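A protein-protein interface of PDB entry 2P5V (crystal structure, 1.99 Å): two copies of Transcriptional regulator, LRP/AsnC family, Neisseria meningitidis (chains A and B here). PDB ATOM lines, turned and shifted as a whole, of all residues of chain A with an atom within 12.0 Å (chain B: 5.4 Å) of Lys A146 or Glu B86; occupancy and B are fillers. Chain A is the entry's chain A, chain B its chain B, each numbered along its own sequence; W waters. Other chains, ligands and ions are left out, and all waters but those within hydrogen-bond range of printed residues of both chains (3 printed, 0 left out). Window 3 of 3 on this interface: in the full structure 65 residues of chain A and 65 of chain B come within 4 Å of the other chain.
Hydrophobic or aromatic side chains of chain B within 4 Å of the printed part of chain A: Ala B89, Phe B102 and Ala B103. Along chain B the printed residues that touch a printed residue of chain A span positions 86 to 103. Of the 20 printed residues of chain A, 8 touch a printed residue of chain B. Printed residues of chain A that touch a printed residue of chain B: Gln A71, Phe A73, Val A144, Leu A145, Lys A146, Glu A147, Ile A148 and Lys A149. Hydrophobic or aromatic side chains of chain A that line the printed part of chain B: Phe A73, Val A144, Leu A145 and Ile A148. Among the printed residues, Asp or Glu carboxylates within 4 Å of a Lys or Arg side-chain nitrogen of the other chain: Lys A146 with Glu B86 (3.8 Å).
No position is printed for both chains. Of the 16 pairs that touch across the chains among the printed residues, none has its exchanged pair printed and touching as well.
Among the printed residues, merely in contact across the chains: Lys A146 with Phe B102 (3.4 Å), Val A144 with Ala B103 (3.6 Å), Val A144 with Phe B102 (3.6 Å), Gln A71 with Phe B102 (3.7 Å), Glu A147 with Phe B102 (3.7 Å), Lys A149 with Arg B93 (3.7 Å), Phe A73 with Phe B102 (3.7 Å), Ile A148 with Ala B103 (3.8 Å), Glu A147 with Cys B101 (3.8 Å) and Ile A148 with Ala B89 (3.8 Å).
Water W2 bridges the side-chain carboxylate of Glu B86 (2.6 Å) and the side-chain amino group of Lys A146 (3.2 Å). Water W1 lies within hydrogen-bond range of the side-chain carboxylate of Glu B86 (2.7 Å), the side-chain amino group of Lys A146 (2.7 Å) and the guanidinium group of Arg B93 (3.4 Å). Water W3 bridges NZ of Lys A149 and O of Arg B93.
The side-chain amide nitrogen (NE2) of Gln A71 lies close to the side-chain amide nitrogen (NE2) of Gln A113, 2.8 Å away. The backbone NH (N) of Phe A73 lies within hydrogen-bond range of the backbone carbonyl oxygen (O) of Ser A142, 2.8 Å away. The backbone carbonyl oxygen (O) of Gln A71 is in hydrogen-bond range of the backbone NH (N) of Val A144, at 3.0 Å.
Of the printed residues of chain A, Glu B86 touches Lys A146 (3.8 Å). No residue of chain A comes within 4 Å of Asp B83. No residue of chain A comes within 4 Å of Ala B84. No residue of chain A comes within 4 Å of Asp B87. Printed residues of chain A within 4 Å of Ala B89: Ile A148. No residue of chain A comes within 4 Å of Ala B90. Of chain A, only Glu A147 (3.8 Å), Ile A148 (2.9 Å) and Lys A149 (2.9 Å) come within 4 Å of Cys B101. Phe B102 touches just these residues of chain A: Gln A71 (3.7 Å), Phe A73 (3.7 Å), Val A144 (3.6 Å), Lys A146 (3.4 Å) and Glu A147 (3.7 Å). Ala B103 touches just these residues of chain A: Val A144, Leu A145, Lys A146 and Ile A148. Of the printed residues of chain B, Lys A149 touches Arg B93 (3.7 Å) and Cys B101 (2.9 Å). Of the printed residues of chain B, Leu A145 touches Ala B103. Ala A72 touches none of the printed residues of chain B. Phe A115 touches none of the printed residues of chain B. The nearest residue of chain B that does not touch Lys A146 is Cys B101 (4.3 Å). The nearest residue of chain A that does not touch Glu B86 is Ile A148 (7.0 Å).
O of Ala B103 lies within hydrogen-bond range of N of Leu A145 (2.9 Å). The backbone NH of Ile A148 sits at hydrogen-bond distance from the backbone carbonyl oxygen of Cys B101 (2.9 Å). The backbone NH (N) of Cys B101 lies within hydrogen-bond range of the backbone carbonyl oxygen (O) of Lys A149 (2.9 Å). The side-chain carboxylate (OE2) of Glu B86 is in salt-bridge range of the side-chain amino group (NZ) of Lys A146, at 3.8 Å. The guanidinium group (NE) of Arg B93 is in hydrogen-bond range of the backbone carbonyl oxygen (O) of Ile A148. O of Lys A146 sits at hydrogen-bond distance from N of Ala B103.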
ATOM      1  N   PRO A  63       5.993 -18.043  -9.281  1.00  0.00           N
ATOM      2  CA  PRO A  63       4.866 -18.924  -8.926  1.00  0.00           C
ATOM      3  C   PRO A  63       5.289 -20.204  -8.208  1.00  0.00           C
ATOM      4  O   PRO A  63       4.635 -20.643  -7.253  1.00  0.00           O
ATOM      5  CB  PRO A  63       4.260 -19.281 -10.286  1.00  0.00           C
ATOM      6  CG  PRO A  63       4.732 -18.213 -11.219  1.00  0.00           C
ATOM      7  CD  PRO A  63       6.063 -17.789 -10.731  1.00  0.00           C
ATOM      8  N   GLU A  64       6.388 -20.785  -8.676  1.00  0.00           N
ATOM      9  CA  GLU A  64       6.885 -22.046  -8.149  1.00  0.00           C
ATOM     10  C   GLU A  64       7.391 -21.835  -6.735  1.00  0.00           C
ATOM     11  O   GLU A  64       7.218 -22.703  -5.884  1.00  0.00           O
ATOM     12  CB  GLU A  64       8.001 -22.606  -9.032  1.00  0.00           C
ATOM     13  CG  GLU A  64       7.635 -22.777 -10.512  1.00  0.00           C
ATOM     14  CD  GLU A  64       7.649 -21.470 -11.310  1.00  0.00           C
ATOM     15  OE1 GLU A  64       7.183 -21.483 -12.472  1.00  0.00           O
ATOM     16  OE2 GLU A  64       8.107 -20.430 -10.784  1.00  0.00           O
ATOM     17  N   LEU A  68       2.679 -22.502  -6.608  1.00  0.00           N
ATOM     18  CA  LEU A  68       1.713 -22.390  -7.699  1.00  0.00           C
ATOM     19  C   LEU A  68       2.342 -23.008  -8.934  1.00  0.00           C
ATOM     20  O   LEU A  68       2.885 -22.316  -9.790  1.00  0.00           O
ATOM     21  CB  LEU A  68       1.308 -20.935  -7.929  1.00  0.00           C
ATOM     22  CG  LEU A  68       0.579 -20.280  -6.744  1.00  0.00           C
ATOM     23  CD1 LEU A  68       0.551 -18.780  -6.910  1.00  0.00           C
ATOM     24  CD2 LEU A  68      -0.839 -20.839  -6.608  1.00  0.00           C
ATOM     25  N   GLY A  69       2.285 -24.335  -8.989  1.00  0.00           N
ATOM     26  CA  GLY A  69       2.876 -25.104 -10.082  1.00  0.00           C
ATOM     27  C   GLY A  69       1.985 -25.273 -11.303  1.00  0.00           C
ATOM     28  O   GLY A  69       2.434 -25.750 -12.341  1.00  0.00           O
ATOM     29  N   LEU A  70       0.719 -24.891 -11.194  1.00  0.00           N
ATOM     30  CA  LEU A  70      -0.189 -25.034 -12.310  1.00  0.00           C
ATOM     31  C   LEU A  70      -0.677 -23.679 -12.802  1.00  0.00           C
ATOM     32  O   LEU A  70      -1.368 -22.954 -12.079  1.00  0.00           O
ATOM     33  CB  LEU A  70      -1.366 -25.922 -11.943  1.00  0.00           C
ATOM     34  CG  LEU A  70      -2.217 -26.347 -13.134  1.00  0.00           C
ATOM     35  CD1 LEU A  70      -1.364 -27.200 -14.071  1.00  0.00           C
ATOM     36  CD2 LEU A  70      -3.463 -27.080 -12.652  1.00  0.00           C
ATOM     37  N   GLN A  71      -0.315 -23.367 -14.046  1.00  0.00           N
ATOM     38  CA  GLN A  71      -0.812 -22.190 -14.737  1.00  0.00           C
ATOM     39  C   GLN A  71      -1.756 -22.609 -15.880  1.00  0.00           C
ATOM     40  O   GLN A  71      -1.410 -23.412 -16.745  1.00  0.00           O
ATOM     41  CB  GLN A  71       0.349 -21.334 -15.250  1.00  0.00           C
ATOM     42  CG  GLN A  71      -0.083 -19.963 -15.742  1.00  0.00           C
ATOM     43  CD  GLN A  71       1.064 -19.116 -16.294  1.00  0.00           C
ATOM     44  OE1 GLN A  71       2.236 -19.489 -16.222  1.00  0.00           O
ATOM     45  NE2 GLN A  71       0.721 -17.966 -16.842  1.00  0.00           N
ATOM     46  N   ALA A  72      -2.943 -22.016 -15.871  1.00  0.00           N
ATOM     47  CA  ALA A  72      -4.028 -22.391 -16.753  1.00  0.00           C
ATOM     48  C   ALA A  72      -4.468 -21.219 -17.625  1.00  0.00           C
ATOM     49  O   ALA A  72      -4.551 -20.063 -17.171  1.00  0.00           O
ATOM     50  CB  ALA A  72      -5.214 -22.884 -15.926  1.00  0.00           C
ATOM     51  N   PHE A  73      -4.761 -21.546 -18.879  1.00  0.00           N
ATOM     52  CA  PHE A  73      -5.461 -20.651 -19.773  1.00  0.00           C
ATOM     53  C   PHE A  73      -6.842 -21.249 -19.956  1.00  0.00           C
ATOM     54  O   PHE A  73      -6.982 -22.373 -20.423  1.00  0.00           O
ATOM     55  CB  PHE A  73      -4.691 -20.513 -21.081  1.00  0.00           C
ATOM     56  CG  PHE A  73      -3.460 -19.660 -20.946  1.00  0.00           C
ATOM     57  CD1 PHE A  73      -3.535 -18.287 -21.127  1.00  0.00           C
ATOM     58  CD2 PHE A  73      -2.243 -20.222 -20.585  1.00  0.00           C
ATOM     59  CE1 PHE A  73      -2.402 -17.477 -20.976  1.00  0.00           C
ATOM     60  CE2 PHE A  73      -1.105 -19.424 -20.435  1.00  0.00           C
ATOM     61  CZ  PHE A  73      -1.193 -18.046 -20.630  1.00  0.00           C
ATOM     62  N   GLN A 113      -6.465 -16.238 -17.347  1.00  0.00           N
ATOM     63  CA  GLN A 113      -5.155 -16.727 -16.968  1.00  0.00           C
ATOM     64  C   GLN A 113      -5.179 -16.856 -15.459  1.00  0.00           C
ATOM     65  O   GLN A 113      -5.452 -15.884 -14.751  1.00  0.00           O
ATOM     66  CB  GLN A 113      -4.049 -15.776 -17.433  1.00  0.00           C
ATOM     67  CG  GLN A 113      -2.646 -16.317 -17.188  1.00  0.00           C
ATOM     68  CD  GLN A 113      -1.547 -15.534 -17.926  1.00  0.00           C
ATOM     69  OE1 GLN A 113      -1.759 -15.003 -19.022  1.00  0.00           O
ATOM     70  NE2 GLN A 113      -0.363 -15.477 -17.321  1.00  0.00           N
ATOM     71  N   PHE A 115      -3.705 -19.201 -11.768  1.00  0.00           N
ATOM     72  CA  PHE A 115      -2.690 -20.022 -11.109  1.00  0.00           C
ATOM     73  C   PHE A 115      -3.293 -20.873 -10.013  1.00  0.00           C
ATOM     74  O   PHE A 115      -4.161 -20.423  -9.257  1.00  0.00           O
ATOM     75  CB  PHE A 115      -1.609 -19.152 -10.486  1.00  0.00           C
ATOM     76  CG  PHE A 115      -0.591 -18.660 -11.462  1.00  0.00           C
ATOM     77  CD1 PHE A 115       0.612 -19.333 -11.634  1.00  0.00           C
ATOM     78  CD2 PHE A 115      -0.832 -17.519 -12.211  1.00  0.00           C
ATOM     79  CE1 PHE A 115       1.566 -18.870 -12.531  1.00  0.00           C
ATOM     80  CE2 PHE A 115       0.121 -17.046 -13.101  1.00  0.00           C
ATOM     81  CZ  PHE A 115       1.318 -17.725 -13.265  1.00  0.00           C
ATOM     82  N   SER A 142      -6.286 -25.094 -21.012  1.00  0.00           N
ATOM     83  CA  SER A 142      -4.995 -25.565 -21.429  1.00  0.00           C
ATOM     84  C   SER A 142      -4.024 -25.120 -20.352  1.00  0.00           C
ATOM     85  O   SER A 142      -4.328 -24.213 -19.563  1.00  0.00           O
ATOM     86  CB  SER A 142      -4.646 -24.977 -22.802  1.00  0.00           C
ATOM     87  OG  SER A 142      -3.517 -25.625 -23.349  1.00  0.00           O
ATOM     88  N   PHE A 143      -2.868 -25.771 -20.294  1.00  0.00           N
ATOM     89  CA  PHE A 143      -1.927 -25.541 -19.203  1.00  0.00           C
ATOM     90  C   PHE A 143      -0.528 -25.326 -19.750  1.00  0.00           C
ATOM     91  O   PHE A 143      -0.179 -25.833 -20.810  1.00  0.00           O
ATOM     92  CB  PHE A 143      -1.990 -26.711 -18.205  1.00  0.00           C
ATOM     93  CG  PHE A 143      -3.392 -27.009 -17.734  1.00  0.00           C
ATOM     94  CD1 PHE A 143      -3.924 -26.357 -16.630  1.00  0.00           C
ATOM     95  CD2 PHE A 143      -4.189 -27.907 -18.423  1.00  0.00           C
ATOM     96  CE1 PHE A 143      -5.222 -26.603 -16.213  1.00  0.00           C
ATOM     97  CE2 PHE A 143      -5.477 -28.164 -18.008  1.00  0.00           C
ATOM     98  CZ  PHE A 143      -5.995 -27.504 -16.897  1.00  0.00           C
ATOM     99  N   VAL A 144       0.251 -24.544 -19.012  1.00  0.00           N
ATOM    100  CA  VAL A 144       1.635 -24.246 -19.362  1.00  0.00           C
ATOM    101  C   VAL A 144       2.563 -25.455 -19.144  1.00  0.00           C
ATOM    102  O   VAL A 144       2.711 -25.958 -18.028  1.00  0.00           O
ATOM    103  CB  VAL A 144       2.159 -23.023 -18.562  1.00  0.00           C
ATOM    104  CG1 VAL A 144       3.677 -22.840 -18.741  1.00  0.00           C
ATOM    105  CG2 VAL A 144       1.413 -21.766 -18.979  1.00  0.00           C
ATOM    106  N   LEU A 145       3.180 -25.897 -20.238  1.00  0.00           N
ATOM    107  CA  LEU A 145       4.235 -26.901 -20.219  1.00  0.00           C
ATOM    108  C   LEU A 145       5.600 -26.267 -20.005  1.00  0.00           C
ATOM    109  O   LEU A 145       6.479 -26.871 -19.396  1.00  0.00           O
ATOM    110  CB  LEU A 145       4.262 -27.653 -21.543  1.00  0.00           C
ATOM    111  CG  LEU A 145       3.067 -28.544 -21.852  1.00  0.00           C
ATOM    112  CD1 LEU A 145       3.313 -29.228 -23.182  1.00  0.00           C
ATOM    113  CD2 LEU A 145       2.838 -29.564 -20.737  1.00  0.00           C
ATOM    114  N   LYS A 146       5.784 -25.062 -20.533  1.00  0.00           N
ATOM    115  CA  LYS A 146       7.050 -24.348 -20.408  1.00  0.00           C
ATOM    116  C   LYS A 146       6.848 -22.863 -20.682  1.00  0.00           C
ATOM    117  O   LYS A 146       6.164 -22.498 -21.634  1.00  0.00           O
ATOM    118  CB  LYS A 146       8.060 -24.911 -21.391  1.00  0.00           C
ATOM    119  CG  LYS A 146       9.492 -24.487 -21.138  1.00  0.00           C
ATOM    120  CD  LYS A 146      10.387 -24.999 -22.239  1.00  0.00           C
ATOM    121  CE  LYS A 146      11.838 -24.595 -22.023  1.00  0.00           C
ATOM    122  NZ  LYS A 146      12.688 -25.018 -23.176  1.00  0.00           N
ATOM    123  N   GLU A 147       7.437 -22.021 -19.835  1.00  0.00           N
ATOM    124  CA  GLU A 147       7.438 -20.581 -20.039  1.00  0.00           C
ATOM    125  C   GLU A 147       8.668 -20.221 -20.835  1.00  0.00           C
ATOM    126  O   GLU A 147       9.781 -20.397 -20.364  1.00  0.00           O
ATOM    127  CB  GLU A 147       7.473 -19.837 -18.712  1.00  0.00           C
ATOM    128  CG  GLU A 147       7.580 -18.331 -18.860  1.00  0.00           C
ATOM    129  CD  GLU A 147       7.698 -17.643 -17.521  1.00  0.00           C
ATOM    130  OE1 GLU A 147       6.717 -17.698 -16.742  1.00  0.00           O
ATOM    131  OE2 GLU A 147       8.769 -17.053 -17.252  1.00  0.00           O
ATOM    132  N   ILE A 148       8.454 -19.707 -22.039  1.00  0.00           N
ATOM    133  CA  ILE A 148       9.543 -19.290 -22.909  1.00  0.00           C
ATOM    134  C   ILE A 148       9.957 -17.842 -22.611  1.00  0.00           C
ATOM    135  O   ILE A 148      11.148 -17.521 -22.578  1.00  0.00           O
ATOM    136  CB  ILE A 148       9.133 -19.467 -24.387  1.00  0.00           C
ATOM    137  CG1 ILE A 148       9.199 -20.958 -24.761  1.00  0.00           C
ATOM    138  CG2 ILE A 148      10.017 -18.647 -25.314  1.00  0.00           C
ATOM    139  CD1 ILE A 148       8.288 -21.848 -23.907  1.00  0.00           C
ATOM    140  N   LYS A 149       8.969 -16.988 -22.365  1.00  0.00           N
ATOM    141  CA  LYS A 149       9.203 -15.565 -22.099  1.00  0.00           C
ATOM    142  C   LYS A 149       8.067 -15.062 -21.239  1.00  0.00           C
ATOM    143  O   LYS A 149       6.946 -15.497 -21.415  1.00  0.00           O
ATOM    144  CB  LYS A 149       9.236 -14.819 -23.425  1.00  0.00           C
ATOM    145  CG  LYS A 149       9.703 -13.388 -23.355  1.00  0.00           C
ATOM    146  CD  LYS A 149       9.678 -12.758 -24.747  1.00  0.00           C
ATOM    147  CE  LYS A 149      10.333 -11.377 -24.765  1.00  0.00           C
ATOM    148  NZ  LYS A 149      10.203 -10.724 -26.098  1.00  0.00           N
ATOM    149  N   HIS A 150       8.355 -14.179 -20.285  1.00  0.00           N
ATOM    150  CA  HIS A 150       7.298 -13.528 -19.518  1.00  0.00           C
ATOM    151  C   HIS A 150       7.847 -12.248 -18.930  1.00  0.00           C
ATOM    152  O   HIS A 150       8.603 -12.279 -17.967  1.00  0.00           O
ATOM    153  CB  HIS A 150       6.770 -14.452 -18.421  1.00  0.00           C
ATOM    154  CG  HIS A 150       5.722 -13.826 -17.552  1.00  0.00           C
ATOM    155  ND1 HIS A 150       4.690 -13.066 -18.057  1.00  0.00           N
ATOM    156  CD2 HIS A 150       5.535 -13.873 -16.215  1.00  0.00           C
ATOM    157  CE1 HIS A 150       3.929 -12.647 -17.065  1.00  0.00           C
ATOM    158  NE2 HIS A 150       4.412 -13.132 -15.936  1.00  0.00           N
ATOM    159  N   THR A 151       7.508 -11.125 -19.544  1.00  0.00           N
ATOM    160  CA  THR A 151       7.883  -9.810 -19.004  1.00  0.00           C
ATOM    161  C   THR A 151       6.655  -8.940 -18.962  1.00  0.00           C
ATOM    162  O   THR A 151       5.693  -9.204 -19.674  1.00  0.00           O
ATOM    163  CB  THR A 151       9.048  -9.128 -19.784  1.00  0.00           C
ATOM    164  OG1 THR A 151       9.282  -7.823 -19.243  1.00  0.00           O
ATOM    165  CG2 THR A 151       8.765  -8.997 -21.252  1.00  0.00           C
ATOM    166  N   ASP B  83      15.505 -28.520 -33.765  1.00  0.00           N
ATOM    167  CA  ASP B  83      15.865 -27.161 -33.340  1.00  0.00           C
ATOM    168  C   ASP B  83      14.826 -26.073 -33.634  1.00  0.00           C
ATOM    169  O   ASP B  83      15.068 -24.913 -33.311  1.00  0.00           O
ATOM    170  CB  ASP B  83      17.236 -26.740 -33.912  1.00  0.00           C
ATOM    171  CG  ASP B  83      18.389 -27.547 -33.334  1.00  0.00           C
ATOM    172  OD1 ASP B  83      18.176 -28.259 -32.327  1.00  0.00           O
ATOM    173  OD2 ASP B  83      19.512 -27.460 -33.884  1.00  0.00           O
ATOM    174  N   ALA B  84      13.676 -26.431 -34.210  1.00  0.00           N
ATOM    175  CA  ALA B  84      12.633 -25.445 -34.506  1.00  0.00           C
ATOM    176  C   ALA B  84      12.134 -24.772 -33.224  1.00  0.00           C
ATOM    177  O   ALA B  84      11.985 -23.547 -33.181  1.00  0.00           O
ATOM    178  CB  ALA B  84      11.474 -26.081 -35.267  1.00  0.00           C
ATOM    179  N   ARG B  85      11.889 -25.566 -32.183  1.00  0.00           N
ATOM    180  CA  ARG B  85      11.358 -25.029 -30.927  1.00  0.00           C
ATOM    181  C   ARG B  85      12.356 -24.086 -30.263  1.00  0.00           C
ATOM    182  O   ARG B  85      11.979 -23.025 -29.751  1.00  0.00           O
ATOM    183  CB  ARG B  85      10.989 -26.153 -29.952  1.00  0.00           C
ATOM    184  CG  ARG B  85       9.691 -26.852 -30.291  1.00  0.00           C
ATOM    185  CD  ARG B  85       9.248 -27.804 -29.214  1.00  0.00           C
ATOM    186  NE  ARG B  85       7.866 -28.242 -29.438  1.00  0.00           N
ATOM    187  CZ  ARG B  85       6.802 -27.898 -28.707  1.00  0.00           C
ATOM    188  NH1 ARG B  85       6.901 -27.102 -27.643  1.00  0.00           N
ATOM    189  NH2 ARG B  85       5.607 -28.374 -29.050  1.00  0.00           N
ATOM    190  N   GLU B  86      13.627 -24.481 -30.270  1.00  0.00           N
ATOM    191  CA  GLU B  86      14.660 -23.708 -29.598  1.00  0.00           C
ATOM    192  C   GLU B  86      15.014 -22.447 -30.369  1.00  0.00           C
ATOM    193  O   GLU B  86      15.217 -21.400 -29.769  1.00  0.00           O
ATOM    194  CB  GLU B  86      15.896 -24.568 -29.335  1.00  0.00           C
ATOM    195  CG  GLU B  86      15.622 -25.709 -28.343  1.00  0.00           C
ATOM    196  CD  GLU B  86      14.896 -25.235 -27.079  1.00  0.00           C
ATOM    197  OE1 GLU B  86      15.423 -24.318 -26.404  1.00  0.00           O
ATOM    198  OE2 GLU B  86      13.801 -25.770 -26.769  1.00  0.00           O
ATOM    199  N   ASP B  87      15.055 -22.547 -31.691  1.00  0.00           N
ATOM    200  CA  ASP B  87      15.266 -21.391 -32.543  1.00  0.00           C
ATOM    201  C   ASP B  87      14.129 -20.398 -32.402  1.00  0.00           C
ATOM    202  O   ASP B  87      14.367 -19.203 -32.391  1.00  0.00           O
ATOM    203  CB  ASP B  87      15.393 -21.820 -33.999  1.00  0.00           C
ATOM    204  CG  ASP B  87      16.592 -22.717 -34.236  1.00  0.00           C
ATOM    205  OD1 ASP B  87      17.459 -22.799 -33.337  1.00  0.00           O
ATOM    206  OD2 ASP B  87      16.649 -23.352 -35.303  1.00  0.00           O
ATOM    207  N   PHE B  88      12.900 -20.900 -32.300  1.00  0.00           N
ATOM    208  CA  PHE B  88      11.729 -20.043 -32.072  1.00  0.00           C
ATOM    209  C   PHE B  88      11.770 -19.348 -30.717  1.00  0.00           C
ATOM    210  O   PHE B  88      11.502 -18.146 -30.617  1.00  0.00           O
ATOM    211  CB  PHE B  88      10.439 -20.846 -32.181  1.00  0.00           C
ATOM    212  CG  PHE B  88       9.213 -20.013 -32.052  1.00  0.00           C
ATOM    213  CD1 PHE B  88       8.890 -19.085 -33.029  1.00  0.00           C
ATOM    214  CD2 PHE B  88       8.378 -20.142 -30.950  1.00  0.00           C
ATOM    215  CE1 PHE B  88       7.751 -18.303 -32.916  1.00  0.00           C
ATOM    216  CE2 PHE B  88       7.237 -19.368 -30.841  1.00  0.00           C
ATOM    217  CZ  PHE B  88       6.927 -18.445 -31.834  1.00  0.00           C
ATOM    218  N   ALA B  89      12.092 -20.112 -29.676  1.00  0.00           N
ATOM    219  CA  ALA B  89      12.246 -19.569 -28.325  1.00  0.00           C
ATOM    220  C   ALA B  89      13.328 -18.478 -28.275  1.00  0.00           C
ATOM    221  O   ALA B  89      13.125 -17.436 -27.659  1.00  0.00           O
ATOM    222  CB  ALA B  89      12.569 -20.694 -27.335  1.00  0.00           C
ATOM    223  N   ALA B  90      14.464 -18.714 -28.928  1.00  0.00           N
ATOM    224  CA  ALA B  90      15.553 -17.721 -28.960  1.00  0.00           C
ATOM    225  C   ALA B  90      15.100 -16.404 -29.603  1.00  0.00           C
ATOM    226  O   ALA B  90      15.357 -15.319 -29.075  1.00  0.00           O
ATOM    227  CB  ALA B  90      16.778 -18.277 -29.695  1.00  0.00           C
ATOM    228  N   SER B  91      14.412 -16.519 -30.735  1.00  0.00           N
ATOM    229  CA  SER B  91      13.907 -15.366 -31.471  1.00  0.00           C
ATOM    230  C   SER B  91      12.834 -14.602 -30.702  1.00  0.00           C
ATOM    231  O   SER B  91      12.884 -13.388 -30.635  1.00  0.00           O
ATOM    232  CB  SER B  91      13.328 -15.817 -32.808  1.00  0.00           C
ATOM    233  OG  SER B  91      14.274 -16.565 -33.559  1.00  0.00           O
ATOM    234  N   ARG B  93      12.394 -14.277 -27.598  1.00  0.00           N
ATOM    235  CA  ARG B  93      13.034 -13.543 -26.503  1.00  0.00           C
ATOM    236  C   ARG B  93      13.676 -12.237 -26.978  1.00  0.00           C
ATOM    237  O   ARG B  93      13.876 -11.322 -26.183  1.00  0.00           O
ATOM    238  CB  ARG B  93      14.080 -14.430 -25.799  1.00  0.00           C
ATOM    239  CG  ARG B  93      13.453 -15.638 -25.118  1.00  0.00           C
ATOM    240  CD  ARG B  93      14.376 -16.379 -24.162  1.00  0.00           C
ATOM    241  NE  ARG B  93      13.721 -17.603 -23.697  1.00  0.00           N
ATOM    242  CZ  ARG B  93      14.018 -18.841 -24.094  1.00  0.00           C
ATOM    243  NH1 ARG B  93      15.014 -19.080 -24.943  1.00  0.00           N
ATOM    244  NH2 ARG B  93      13.328 -19.864 -23.604  1.00  0.00           N
ATOM    245  N   CYS B 101       5.238 -15.838 -23.779  1.00  0.00           N
ATOM    246  CA  CYS B 101       5.192 -16.965 -24.698  1.00  0.00           C
ATOM    247  C   CYS B 101       5.217 -18.226 -23.855  1.00  0.00           C
ATOM    248  O   CYS B 101       6.111 -18.390 -23.021  1.00  0.00           O
ATOM    249  CB  CYS B 101       6.408 -16.943 -25.627  1.00  0.00           C
ATOM    250  SG  CYS B 101       6.428 -18.317 -26.805  1.00  0.00           S
ATOM    251  N   PHE B 102       4.224 -19.087 -24.049  1.00  0.00           N
ATOM    252  CA  PHE B 102       4.091 -20.316 -23.293  1.00  0.00           C
ATOM    253  C   PHE B 102       3.799 -21.467 -24.237  1.00  0.00           C
ATOM    254  O   PHE B 102       2.920 -21.371 -25.077  1.00  0.00           O
ATOM    255  CB  PHE B 102       2.943 -20.235 -22.286  1.00  0.00           C
ATOM    256  CG  PHE B 102       3.065 -19.105 -21.303  1.00  0.00           C
ATOM    257  CD1 PHE B 102       3.797 -19.257 -20.133  1.00  0.00           C
ATOM    258  CD2 PHE B 102       2.422 -17.907 -21.525  1.00  0.00           C
ATOM    259  CE1 PHE B 102       3.902 -18.219 -19.215  1.00  0.00           C
ATOM    260  CE2 PHE B 102       2.525 -16.862 -20.610  1.00  0.00           C
ATOM    261  CZ  PHE B 102       3.258 -17.022 -19.455  1.00  0.00           C
ATOM    262  N   ALA B 103       4.563 -22.543 -24.097  1.00  0.00           N
ATOM    263  CA  ALA B 103       4.230 -23.810 -24.709  1.00  0.00           C
ATOM    264  C   ALA B 103       3.079 -24.365 -23.891  1.00  0.00           C
ATOM    265  O   ALA B 103       3.158 -24.365 -22.662  1.00  0.00           O
ATOM    266  CB  ALA B 103       5.420 -24.734 -24.680  1.00  0.00           C
HETATM  267  O   HOH W   1      14.029 -23.035 -24.508  1.00  0.00           O
HETATM  268  O   HOH W   2      11.925 -24.115 -26.149  1.00  0.00           O
HETATM  269  O   HOH W   3      12.398  -8.793 -26.033  1.00  0.00           O
